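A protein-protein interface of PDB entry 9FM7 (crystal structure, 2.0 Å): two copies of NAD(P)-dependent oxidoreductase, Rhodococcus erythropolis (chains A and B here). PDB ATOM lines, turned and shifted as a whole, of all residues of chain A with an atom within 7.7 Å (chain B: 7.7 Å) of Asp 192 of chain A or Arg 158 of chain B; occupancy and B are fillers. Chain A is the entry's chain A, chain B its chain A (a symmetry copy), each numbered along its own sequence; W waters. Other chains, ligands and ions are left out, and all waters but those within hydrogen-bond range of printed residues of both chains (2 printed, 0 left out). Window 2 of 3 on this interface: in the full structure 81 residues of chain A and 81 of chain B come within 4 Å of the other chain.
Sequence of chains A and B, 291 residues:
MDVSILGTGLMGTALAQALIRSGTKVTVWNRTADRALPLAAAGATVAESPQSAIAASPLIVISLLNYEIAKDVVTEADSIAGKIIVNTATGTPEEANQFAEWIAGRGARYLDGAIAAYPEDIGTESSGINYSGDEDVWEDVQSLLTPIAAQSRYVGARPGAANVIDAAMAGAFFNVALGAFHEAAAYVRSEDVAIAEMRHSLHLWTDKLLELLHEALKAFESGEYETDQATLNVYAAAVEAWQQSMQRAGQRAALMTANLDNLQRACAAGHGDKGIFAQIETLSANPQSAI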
ATOM      1  N   ALA A 186      34.919  20.907  -5.041  1.00  0.00           N
ATOM      2  CA  ALA A 186      35.643  21.770  -4.118  1.00  0.00           C
ATOM      3  C   ALA A 186      34.646  22.602  -3.317  1.00  0.00           C
ATOM      4  O   ALA A 186      34.834  22.810  -2.117  1.00  0.00           O
ATOM      5  CB  ALA A 186      36.613  22.657  -4.860  1.00  0.00           C
ATOM      6  N   TYR A 187      33.574  23.048  -3.986  1.00  0.00           N
ATOM      7  CA  TYR A 187      32.508  23.761  -3.299  1.00  0.00           C
ATOM      8  C   TYR A 187      31.869  22.879  -2.218  1.00  0.00           C
ATOM      9  O   TYR A 187      31.727  23.302  -1.083  1.00  0.00           O
ATOM     10  CB  TYR A 187      31.445  24.285  -4.265  1.00  0.00           C
ATOM     11  CG  TYR A 187      30.232  24.825  -3.519  1.00  0.00           C
ATOM     12  CD1 TYR A 187      30.368  25.831  -2.562  1.00  0.00           C
ATOM     13  CD2 TYR A 187      28.962  24.307  -3.738  1.00  0.00           C
ATOM     14  CE1 TYR A 187      29.274  26.303  -1.849  1.00  0.00           C
ATOM     15  CE2 TYR A 187      27.856  24.781  -3.039  1.00  0.00           C
ATOM     16  CZ  TYR A 187      28.012  25.771  -2.081  1.00  0.00           C
ATOM     17  OH  TYR A 187      26.927  26.219  -1.384  1.00  0.00           O
ATOM     18  N   VAL A 188      31.450  21.665  -2.565  1.00  0.00           N
ATOM     19  CA  VAL A 188      30.824  20.773  -1.605  1.00  0.00           C
ATOM     20  C   VAL A 188      31.746  20.592  -0.400  1.00  0.00           C
ATOM     21  O   VAL A 188      31.297  20.614   0.747  1.00  0.00           O
ATOM     22  CB  VAL A 188      30.486  19.429  -2.279  1.00  0.00           C
ATOM     23  CG1 VAL A 188      30.092  18.348  -1.268  1.00  0.00           C
ATOM     24  CG2 VAL A 188      29.391  19.600  -3.334  1.00  0.00           C
ATOM     25  N   ARG A 189      33.036  20.372  -0.657  1.00  0.00           N
ATOM     26  CA  ARG A 189      33.966  20.096   0.424  1.00  0.00           C
ATOM     27  C   ARG A 189      34.102  21.329   1.311  1.00  0.00           C
ATOM     28  O   ARG A 189      34.120  21.194   2.522  1.00  0.00           O
ATOM     29  CB  ARG A 189      35.284  19.591  -0.160  1.00  0.00           C
ATOM     30  CG  ARG A 189      36.217  18.990   0.876  1.00  0.00           C
ATOM     31  CD  ARG A 189      37.463  18.427   0.196  1.00  0.00           C
ATOM     32  NE  ARG A 189      38.234  19.498  -0.451  1.00  0.00           N
ATOM     33  CZ  ARG A 189      39.231  19.334  -1.322  1.00  0.00           C
ATOM     34  NH1 ARG A 189      39.632  18.116  -1.653  1.00  0.00           N
ATOM     35  NH2 ARG A 189      39.820  20.391  -1.852  1.00  0.00           N
ATOM     36  N   SER A 190      34.090  22.530   0.712  1.00  0.00           N
ATOM     37  CA  SER A 190      34.181  23.790   1.438  1.00  0.00           C
ATOM     38  C   SER A 190      33.011  24.018   2.400  1.00  0.00           C
ATOM     39  O   SER A 190      33.142  24.818   3.321  1.00  0.00           O
ATOM     40  CB  SER A 190      34.343  24.971   0.482  1.00  0.00           C
ATOM     41  OG  SER A 190      33.143  25.309  -0.211  1.00  0.00           O
ATOM     42  N   GLU A 191      31.873  23.340   2.181  1.00  0.00           N
ATOM     43  CA  GLU A 191      30.661  23.522   2.965  1.00  0.00           C
ATOM     44  C   GLU A 191      30.583  22.391   3.989  1.00  0.00           C
ATOM     45  O   GLU A 191      29.519  22.128   4.563  1.00  0.00           O
ATOM     46  CB  GLU A 191      29.423  23.514   2.054  1.00  0.00           C
ATOM     47  CG  GLU A 191      29.275  24.702   1.098  1.00  0.00           C
ATOM     48  CD  GLU A 191      28.672  25.965   1.707  1.00  0.00           C
ATOM     49  OE1 GLU A 191      28.811  26.049   2.931  1.00  0.00           O
ATOM     50  OE2 GLU A 191      28.049  26.826   1.029  1.00  0.00           O
ATOM     51  N   ASP A 192      31.713  21.674   4.140  1.00  0.00           N
ATOM     52  CA  ASP A 192      31.836  20.531   5.040  1.00  0.00           C
ATOM     53  C   ASP A 192      30.790  19.464   4.750  1.00  0.00           C
ATOM     54  O   ASP A 192      30.318  18.805   5.671  1.00  0.00           O
ATOM     55  CB  ASP A 192      31.810  20.964   6.497  1.00  0.00           C
ATOM     56  CG  ASP A 192      33.017  21.806   6.874  1.00  0.00           C
ATOM     57  OD1 ASP A 192      34.156  21.296   6.701  1.00  0.00           O
ATOM     58  OD2 ASP A 192      32.812  22.972   7.283  1.00  0.00           O
ATOM     59  N   VAL A 193      30.478  19.258   3.467  1.00  0.00           N
ATOM     60  CA  VAL A 193      29.586  18.180   3.071  1.00  0.00           C
ATOM     61  C   VAL A 193      30.434  17.097   2.414  1.00  0.00           C
ATOM     62  O   VAL A 193      31.435  17.421   1.784  1.00  0.00           O
ATOM     63  CB  VAL A 193      28.503  18.761   2.140  1.00  0.00           C
ATOM     64  CG1 VAL A 193      27.676  17.687   1.443  1.00  0.00           C
ATOM     65  CG2 VAL A 193      27.569  19.702   2.883  1.00  0.00           C
ATOM     66  N   ALA A 194      30.031  15.824   2.543  1.00  0.00           N
ATOM     67  CA  ALA A 194      30.803  14.712   2.006  1.00  0.00           C
ATOM     68  C   ALA A 194      30.781  14.697   0.472  1.00  0.00           C
ATOM     69  O   ALA A 194      29.740  14.568  -0.143  1.00  0.00           O
ATOM     70  CB  ALA A 194      30.266  13.407   2.546  1.00  0.00           C
ATOM     71  N   ILE A 195      31.951  14.765  -0.149  1.00  0.00           N
ATOM     72  CA  ILE A 195      32.030  14.742  -1.599  1.00  0.00           C
ATOM     73  C   ILE A 195      31.437  13.428  -2.119  1.00  0.00           C
ATOM     74  O   ILE A 195      30.906  13.387  -3.212  1.00  0.00           O
ATOM     75  CB  ILE A 195      33.487  14.991  -2.018  1.00  0.00           C
ATOM     76  CG1 ILE A 195      33.699  16.456  -2.369  1.00  0.00           C
ATOM     77  CG2 ILE A 195      33.938  14.067  -3.147  1.00  0.00           C
ATOM     78  CD1 ILE A 195      35.132  16.780  -2.740  1.00  0.00           C
ATOM     79  N   PRO B  93      22.176  26.692   1.619  1.00  0.00           N
ATOM     80  CA  PRO B  93      22.307  25.909   2.833  1.00  0.00           C
ATOM     81  C   PRO B  93      21.831  26.671   4.067  1.00  0.00           C
ATOM     82  O   PRO B  93      21.325  26.053   4.989  1.00  0.00           O
ATOM     83  CB  PRO B  93      23.802  25.559   2.943  1.00  0.00           C
ATOM     84  CG  PRO B  93      24.485  26.318   1.844  1.00  0.00           C
ATOM     85  CD  PRO B  93      23.438  26.827   0.888  1.00  0.00           C
ATOM     86  N   ALA B  96      18.138  26.541   4.492  1.00  0.00           N
ATOM     87  CA  ALA B  96      17.734  25.256   5.047  1.00  0.00           C
ATOM     88  C   ALA B  96      17.975  25.206   6.551  1.00  0.00           C
ATOM     89  O   ALA B  96      17.127  24.739   7.312  1.00  0.00           O
ATOM     90  CB  ALA B  96      18.461  24.143   4.337  1.00  0.00           C
ATOM     91  N   ASN B  97      19.136  25.689   6.995  1.00  0.00           N
ATOM     92  CA  ASN B  97      19.509  25.576   8.394  1.00  0.00           C
ATOM     93  C   ASN B  97      18.538  26.404   9.221  1.00  0.00           C
ATOM     94  O   ASN B  97      18.102  25.972  10.279  1.00  0.00           O
ATOM     95  CB  ASN B  97      20.959  25.982   8.618  1.00  0.00           C
ATOM     96  CG  ASN B  97      21.467  25.586   9.987  1.00  0.00           C
ATOM     97  OD1 ASN B  97      20.777  24.893  10.750  1.00  0.00           O
ATOM     98  ND2 ASN B  97      22.688  25.990  10.314  1.00  0.00           N
ATOM     99  N   ALA B 100      14.937  24.893   9.231  1.00  0.00           N
ATOM    100  CA  ALA B 100      15.007  23.763  10.140  1.00  0.00           C
ATOM    101  C   ALA B 100      14.832  24.221  11.585  1.00  0.00           C
ATOM    102  O   ALA B 100      14.004  23.687  12.298  1.00  0.00           O
ATOM    103  CB  ALA B 100      16.319  23.031   9.942  1.00  0.00           C
ATOM    104  N   ASP B 112      14.978  18.259   4.880  1.00  0.00           N
ATOM    105  CA  ASP B 112      15.117  19.154   3.749  1.00  0.00           C
ATOM    106  C   ASP B 112      15.416  18.327   2.509  1.00  0.00           C
ATOM    107  O   ASP B 112      16.191  17.373   2.581  1.00  0.00           O
ATOM    108  CB  ASP B 112      16.236  20.153   3.956  1.00  0.00           C
ATOM    109  CG  ASP B 112      16.182  21.342   3.021  1.00  0.00           C
ATOM    110  OD1 ASP B 112      16.671  21.210   1.864  1.00  0.00           O
ATOM    111  OD2 ASP B 112      15.569  22.362   3.439  1.00  0.00           O
ATOM    112  N   TYR B 131      17.933  14.130   0.423  1.00  0.00           N
ATOM    113  CA  TYR B 131      17.343  14.619   1.666  1.00  0.00           C
ATOM    114  C   TYR B 131      18.427  14.810   2.723  1.00  0.00           C
ATOM    115  O   TYR B 131      19.393  14.063   2.744  1.00  0.00           O
ATOM    116  CB  TYR B 131      16.321  13.636   2.223  1.00  0.00           C
ATOM    117  CG  TYR B 131      15.128  13.370   1.320  1.00  0.00           C
ATOM    118  CD1 TYR B 131      14.055  14.247   1.293  1.00  0.00           C
ATOM    119  CD2 TYR B 131      15.049  12.214   0.544  1.00  0.00           C
ATOM    120  CE1 TYR B 131      12.954  14.014   0.490  1.00  0.00           C
ATOM    121  CE2 TYR B 131      13.937  11.954  -0.241  1.00  0.00           C
ATOM    122  CZ  TYR B 131      12.887  12.865  -0.277  1.00  0.00           C
ATOM    123  OH  TYR B 131      11.768  12.673  -1.058  1.00  0.00           O
ATOM    124  N   SER B 132      18.273  15.806   3.603  1.00  0.00           N
ATOM    125  CA  SER B 132      19.266  16.057   4.634  1.00  0.00           C
ATOM    126  C   SER B 132      18.609  16.679   5.870  1.00  0.00           C
ATOM    127  O   SER B 132      17.571  17.331   5.784  1.00  0.00           O
ATOM    128  CB  SER B 132      20.390  16.950   4.131  1.00  0.00           C
ATOM    129  OG  SER B 132      19.858  18.154   3.593  1.00  0.00           O
ATOM    130  N   GLY B 133      19.274  16.495   7.012  1.00  0.00           N
ATOM    131  CA  GLY B 133      18.726  16.884   8.295  1.00  0.00           C
ATOM    132  C   GLY B 133      18.721  15.675   9.230  1.00  0.00           C
ATOM    133  O   GLY B 133      19.563  14.779   9.110  1.00  0.00           O
ATOM    134  N   ASP B 134      17.694  15.616  10.073  1.00  0.00           N
ATOM    135  CA  ASP B 134      17.598  14.599  11.104  1.00  0.00           C
ATOM    136  C   ASP B 134      17.323  13.240  10.459  1.00  0.00           C
ATOM    137  O   ASP B 134      16.246  12.987   9.889  1.00  0.00           O
ATOM    138  CB  ASP B 134      16.550  14.970  12.150  1.00  0.00           C
ATOM    139  CG  ASP B 134      16.596  16.396  12.698  1.00  0.00           C
ATOM    140  OD1 ASP B 134      16.357  17.342  11.920  1.00  0.00           O
ATOM    141  OD2 ASP B 134      16.856  16.561  13.901  1.00  0.00           O
ATOM    142  N   TYR B 154      19.498   9.839   1.551  1.00  0.00           N
ATOM    143  CA  TYR B 154      19.865  10.691   2.676  1.00  0.00           C
ATOM    144  C   TYR B 154      21.356  11.025   2.578  1.00  0.00           C
ATOM    145  O   TYR B 154      22.172  10.116   2.573  1.00  0.00           O
ATOM    146  CB  TYR B 154      19.474   9.945   3.960  1.00  0.00           C
ATOM    147  CG  TYR B 154      19.916  10.667   5.224  1.00  0.00           C
ATOM    148  CD1 TYR B 154      19.179  11.726   5.726  1.00  0.00           C
ATOM    149  CD2 TYR B 154      21.082  10.316   5.892  1.00  0.00           C
ATOM    150  CE1 TYR B 154      19.583  12.401   6.866  1.00  0.00           C
ATOM    151  CE2 TYR B 154      21.494  10.977   7.042  1.00  0.00           C
ATOM    152  CZ  TYR B 154      20.750  12.037   7.524  1.00  0.00           C
ATOM    153  OH  TYR B 154      21.135  12.705   8.655  1.00  0.00           O
ATOM    154  N   VAL B 155      21.709  12.319   2.495  1.00  0.00           N
ATOM    155  CA  VAL B 155      23.060  12.735   2.147  1.00  0.00           C
ATOM    156  C   VAL B 155      23.750  13.486   3.291  1.00  0.00           C
ATOM    157  O   VAL B 155      24.852  14.002   3.101  1.00  0.00           O
ATOM    158  CB  VAL B 155      23.067  13.614   0.885  1.00  0.00           C
ATOM    159  CG1 VAL B 155      22.498  12.868  -0.316  1.00  0.00           C
ATOM    160  CG2 VAL B 155      22.341  14.929   1.101  1.00  0.00           C
ATOM    161  N   GLY B 156      23.137  13.569   4.481  1.00  0.00           N
ATOM    162  CA  GLY B 156      23.867  14.151   5.594  1.00  0.00           C
ATOM    163  C   GLY B 156      22.960  14.729   6.669  1.00  0.00           C
ATOM    164  O   GLY B 156      21.773  14.975   6.431  1.00  0.00           O
ATOM    165  N   ALA B 157      23.581  14.964   7.836  1.00  0.00           N
ATOM    166  CA  ALA B 157      22.926  15.475   9.032  1.00  0.00           C
ATOM    167  C   ALA B 157      22.684  16.980   8.923  1.00  0.00           C
ATOM    168  O   ALA B 157      21.683  17.482   9.439  1.00  0.00           O
ATOM    169  CB  ALA B 157      23.772  15.145  10.252  1.00  0.00           C
ATOM    170  N   ARG B 158      23.563  17.720   8.232  1.00  0.00           N
ATOM    171  CA  ARG B 158      23.357  19.163   8.081  1.00  0.00           C
ATOM    172  C   ARG B 158      22.088  19.440   7.263  1.00  0.00           C
ATOM    173  O   ARG B 158      21.955  18.946   6.143  1.00  0.00           O
ATOM    174  CB  ARG B 158      24.602  19.769   7.422  1.00  0.00           C
ATOM    175  CG  ARG B 158      24.710  21.285   7.347  1.00  0.00           C
ATOM    176  CD  ARG B 158      26.093  21.765   6.843  1.00  0.00           C
ATOM    177  NE  ARG B 158      27.190  20.898   7.300  1.00  0.00           N
ATOM    178  CZ  ARG B 158      28.187  21.212   8.135  1.00  0.00           C
ATOM    179  NH1 ARG B 158      28.367  22.463   8.535  1.00  0.00           N
ATOM    180  NH2 ARG B 158      29.029  20.269   8.544  1.00  0.00           N
ATOM    181  N   PRO B 159      21.104  20.215   7.776  1.00  0.00           N
ATOM    182  CA  PRO B 159      19.903  20.551   7.000  1.00  0.00           C
ATOM    183  C   PRO B 159      20.224  21.022   5.584  1.00  0.00           C
ATOM    184  O   PRO B 159      19.511  20.735   4.621  1.00  0.00           O
ATOM    185  CB  PRO B 159      19.274  21.681   7.841  1.00  0.00           C
ATOM    186  CG  PRO B 159      19.645  21.296   9.269  1.00  0.00           C
ATOM    187  CD  PRO B 159      21.062  20.761   9.145  1.00  0.00           C
ATOM    188  N   GLY B 160      21.330  21.750   5.466  1.00  0.00           N
ATOM    189  CA  GLY B 160      21.683  22.374   4.208  1.00  0.00           C
ATOM    190  C   GLY B 160      22.466  21.482   3.236  1.00  0.00           C
ATOM    191  O   GLY B 160      22.860  21.999   2.196  1.00  0.00           O
ATOM    192  N   ALA B 161      22.727  20.197   3.540  1.00  0.00           N
ATOM    193  CA  ALA B 161      23.591  19.383   2.675  1.00  0.00           C
ATOM    194  C   ALA B 161      22.977  19.149   1.296  1.00  0.00           C
ATOM    195  O   ALA B 161      23.692  19.163   0.294  1.00  0.00           O
ATOM    196  CB  ALA B 161      23.935  18.054   3.306  1.00  0.00           C
ATOM    197  N   ALA B 162      21.666  18.908   1.241  1.00  0.00           N
ATOM    198  CA  ALA B 162      21.028  18.634  -0.041  1.00  0.00           C
ATOM    199  C   ALA B 162      21.096  19.878  -0.935  1.00  0.00           C
ATOM    200  O   ALA B 162      21.294  19.797  -2.161  1.00  0.00           O
ATOM    201  CB  ALA B 162      19.603  18.154   0.164  1.00  0.00           C
ATOM    202  N   ASN B 163      20.911  21.031  -0.310  1.00  0.00           N
ATOM    203  CA  ASN B 163      20.956  22.285  -1.051  1.00  0.00           C
ATOM    204  C   ASN B 163      22.382  22.547  -1.541  1.00  0.00           C
ATOM    205  O   ASN B 163      22.545  23.146  -2.596  1.00  0.00           O
ATOM    206  CB  ASN B 163      20.469  23.462  -0.212  1.00  0.00           C
ATOM    207  CG  ASN B 163      18.975  23.562  -0.095  1.00  0.00           C
ATOM    208  OD1 ASN B 163      18.205  22.775  -0.677  1.00  0.00           O
ATOM    209  ND2 ASN B 163      18.540  24.549   0.673  1.00  0.00           N
ATOM    210  N   VAL B 164      23.409  22.154  -0.757  1.00  0.00           N
ATOM    211  CA  VAL B 164      24.794  22.346  -1.183  1.00  0.00           C
ATOM    212  C   VAL B 164      25.070  21.465  -2.403  1.00  0.00           C
ATOM    213  O   VAL B 164      25.580  21.934  -3.412  1.00  0.00           O
ATOM    214  CB  VAL B 164      25.800  22.044  -0.066  1.00  0.00           C
ATOM    215  CG1 VAL B 164      27.230  21.922  -0.575  1.00  0.00           C
ATOM    216  CG2 VAL B 164      25.721  23.075   1.038  1.00  0.00           C
HETATM  217  O   HOH W   1      30.546  24.674   7.126  1.00  0.00           O
HETATM  218  O   HOH W   2      27.228  15.219   4.007  1.00  0.00           O
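Along chain B the printed residues that touch a printed residue of chain A span positions 93 to 164.
Of the 10 printed residues of chain A, 5 touch a printed residue of chain B.
Hydrophobic or aromatic side chains of chain A within 4 Å of the printed part of chain B: Tyr 187 and Val 193.
Among the printed residues, no Asp or Glu carboxylate lies within 4 Å of a Lys or Arg side-chain nitrogen of the other chain.
Asp 192 of chain A touches just one residue of chain B: Arg 158 (3.5 Å).
Of chain A, only Glu 191 and Asp 192 come within 4 Å of Arg 158 of chain B.
Of the printed residues of chain A, Pro 93 of chain B touches Glu 191.
Printed residues of chain A within 4 Å of Ala 161 of chain B: Val 193 (3.996 Å).
Of the printed residues of chain A, Val 164 of chain B touches Tyr 187 (3.7 Å), Val 188 (3.9 Å) and Glu 191 (3.8 Å).
Of the printed residues of chain B, Val 188 of chain A touches Val 164 (3.9 Å).
The side-chain hydroxyl of Tyr 187 of chain A is in hydrogen-bond range of the side-chain carboxylate of Glu 191 of chain A (2.7 Å).
The backbone NH of Val 193 of chain A is in hydrogen-bond range of the backbone carbonyl oxygen of Val 188 of chain A (3.1 Å).
O of Tyr 187 of chain A lies within hydrogen-bond range of OG of Ser 190 of chain A, 2.6 Å away.
O of Arg 158 of chain B sits close to OG of Ser 132 of chain B, at 3.4 Å.
No position is printed for both chains.
O of Asp 192 of chain A is in hydrogen-bond range of NH2 of Arg 158 of chain B (3.5 Å).
Water W2 bridges O of Val 155 of chain B (2.8 Å) and N of Ala 194 of chain A (3.2 Å).
Water W1 lies within hydrogen-bond range of the side-chain carboxylate of Asp 192 of chain A (2.8 Å) and the guanidinium group of Arg 158 of chain B (3.4 Å).
CE2 of Tyr 187 of chain A touches O of Val 164 of chain B, 3.7 Å away.
CA of Val 188 of chain A touches CG1 of Val 164 of chain B, at 3.9 Å.
Glu 191 of chain A touches Pro 93 of chain B (OE2 to CG, 3.7 Å).
NE of Arg 158 of chain B touches O of Glu 191 of chain A, 3.8 Å away.
Glu 191 of chain A touches Val 164 of chain B.
Val 193 of chain A touches Ala 161 of chain B.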
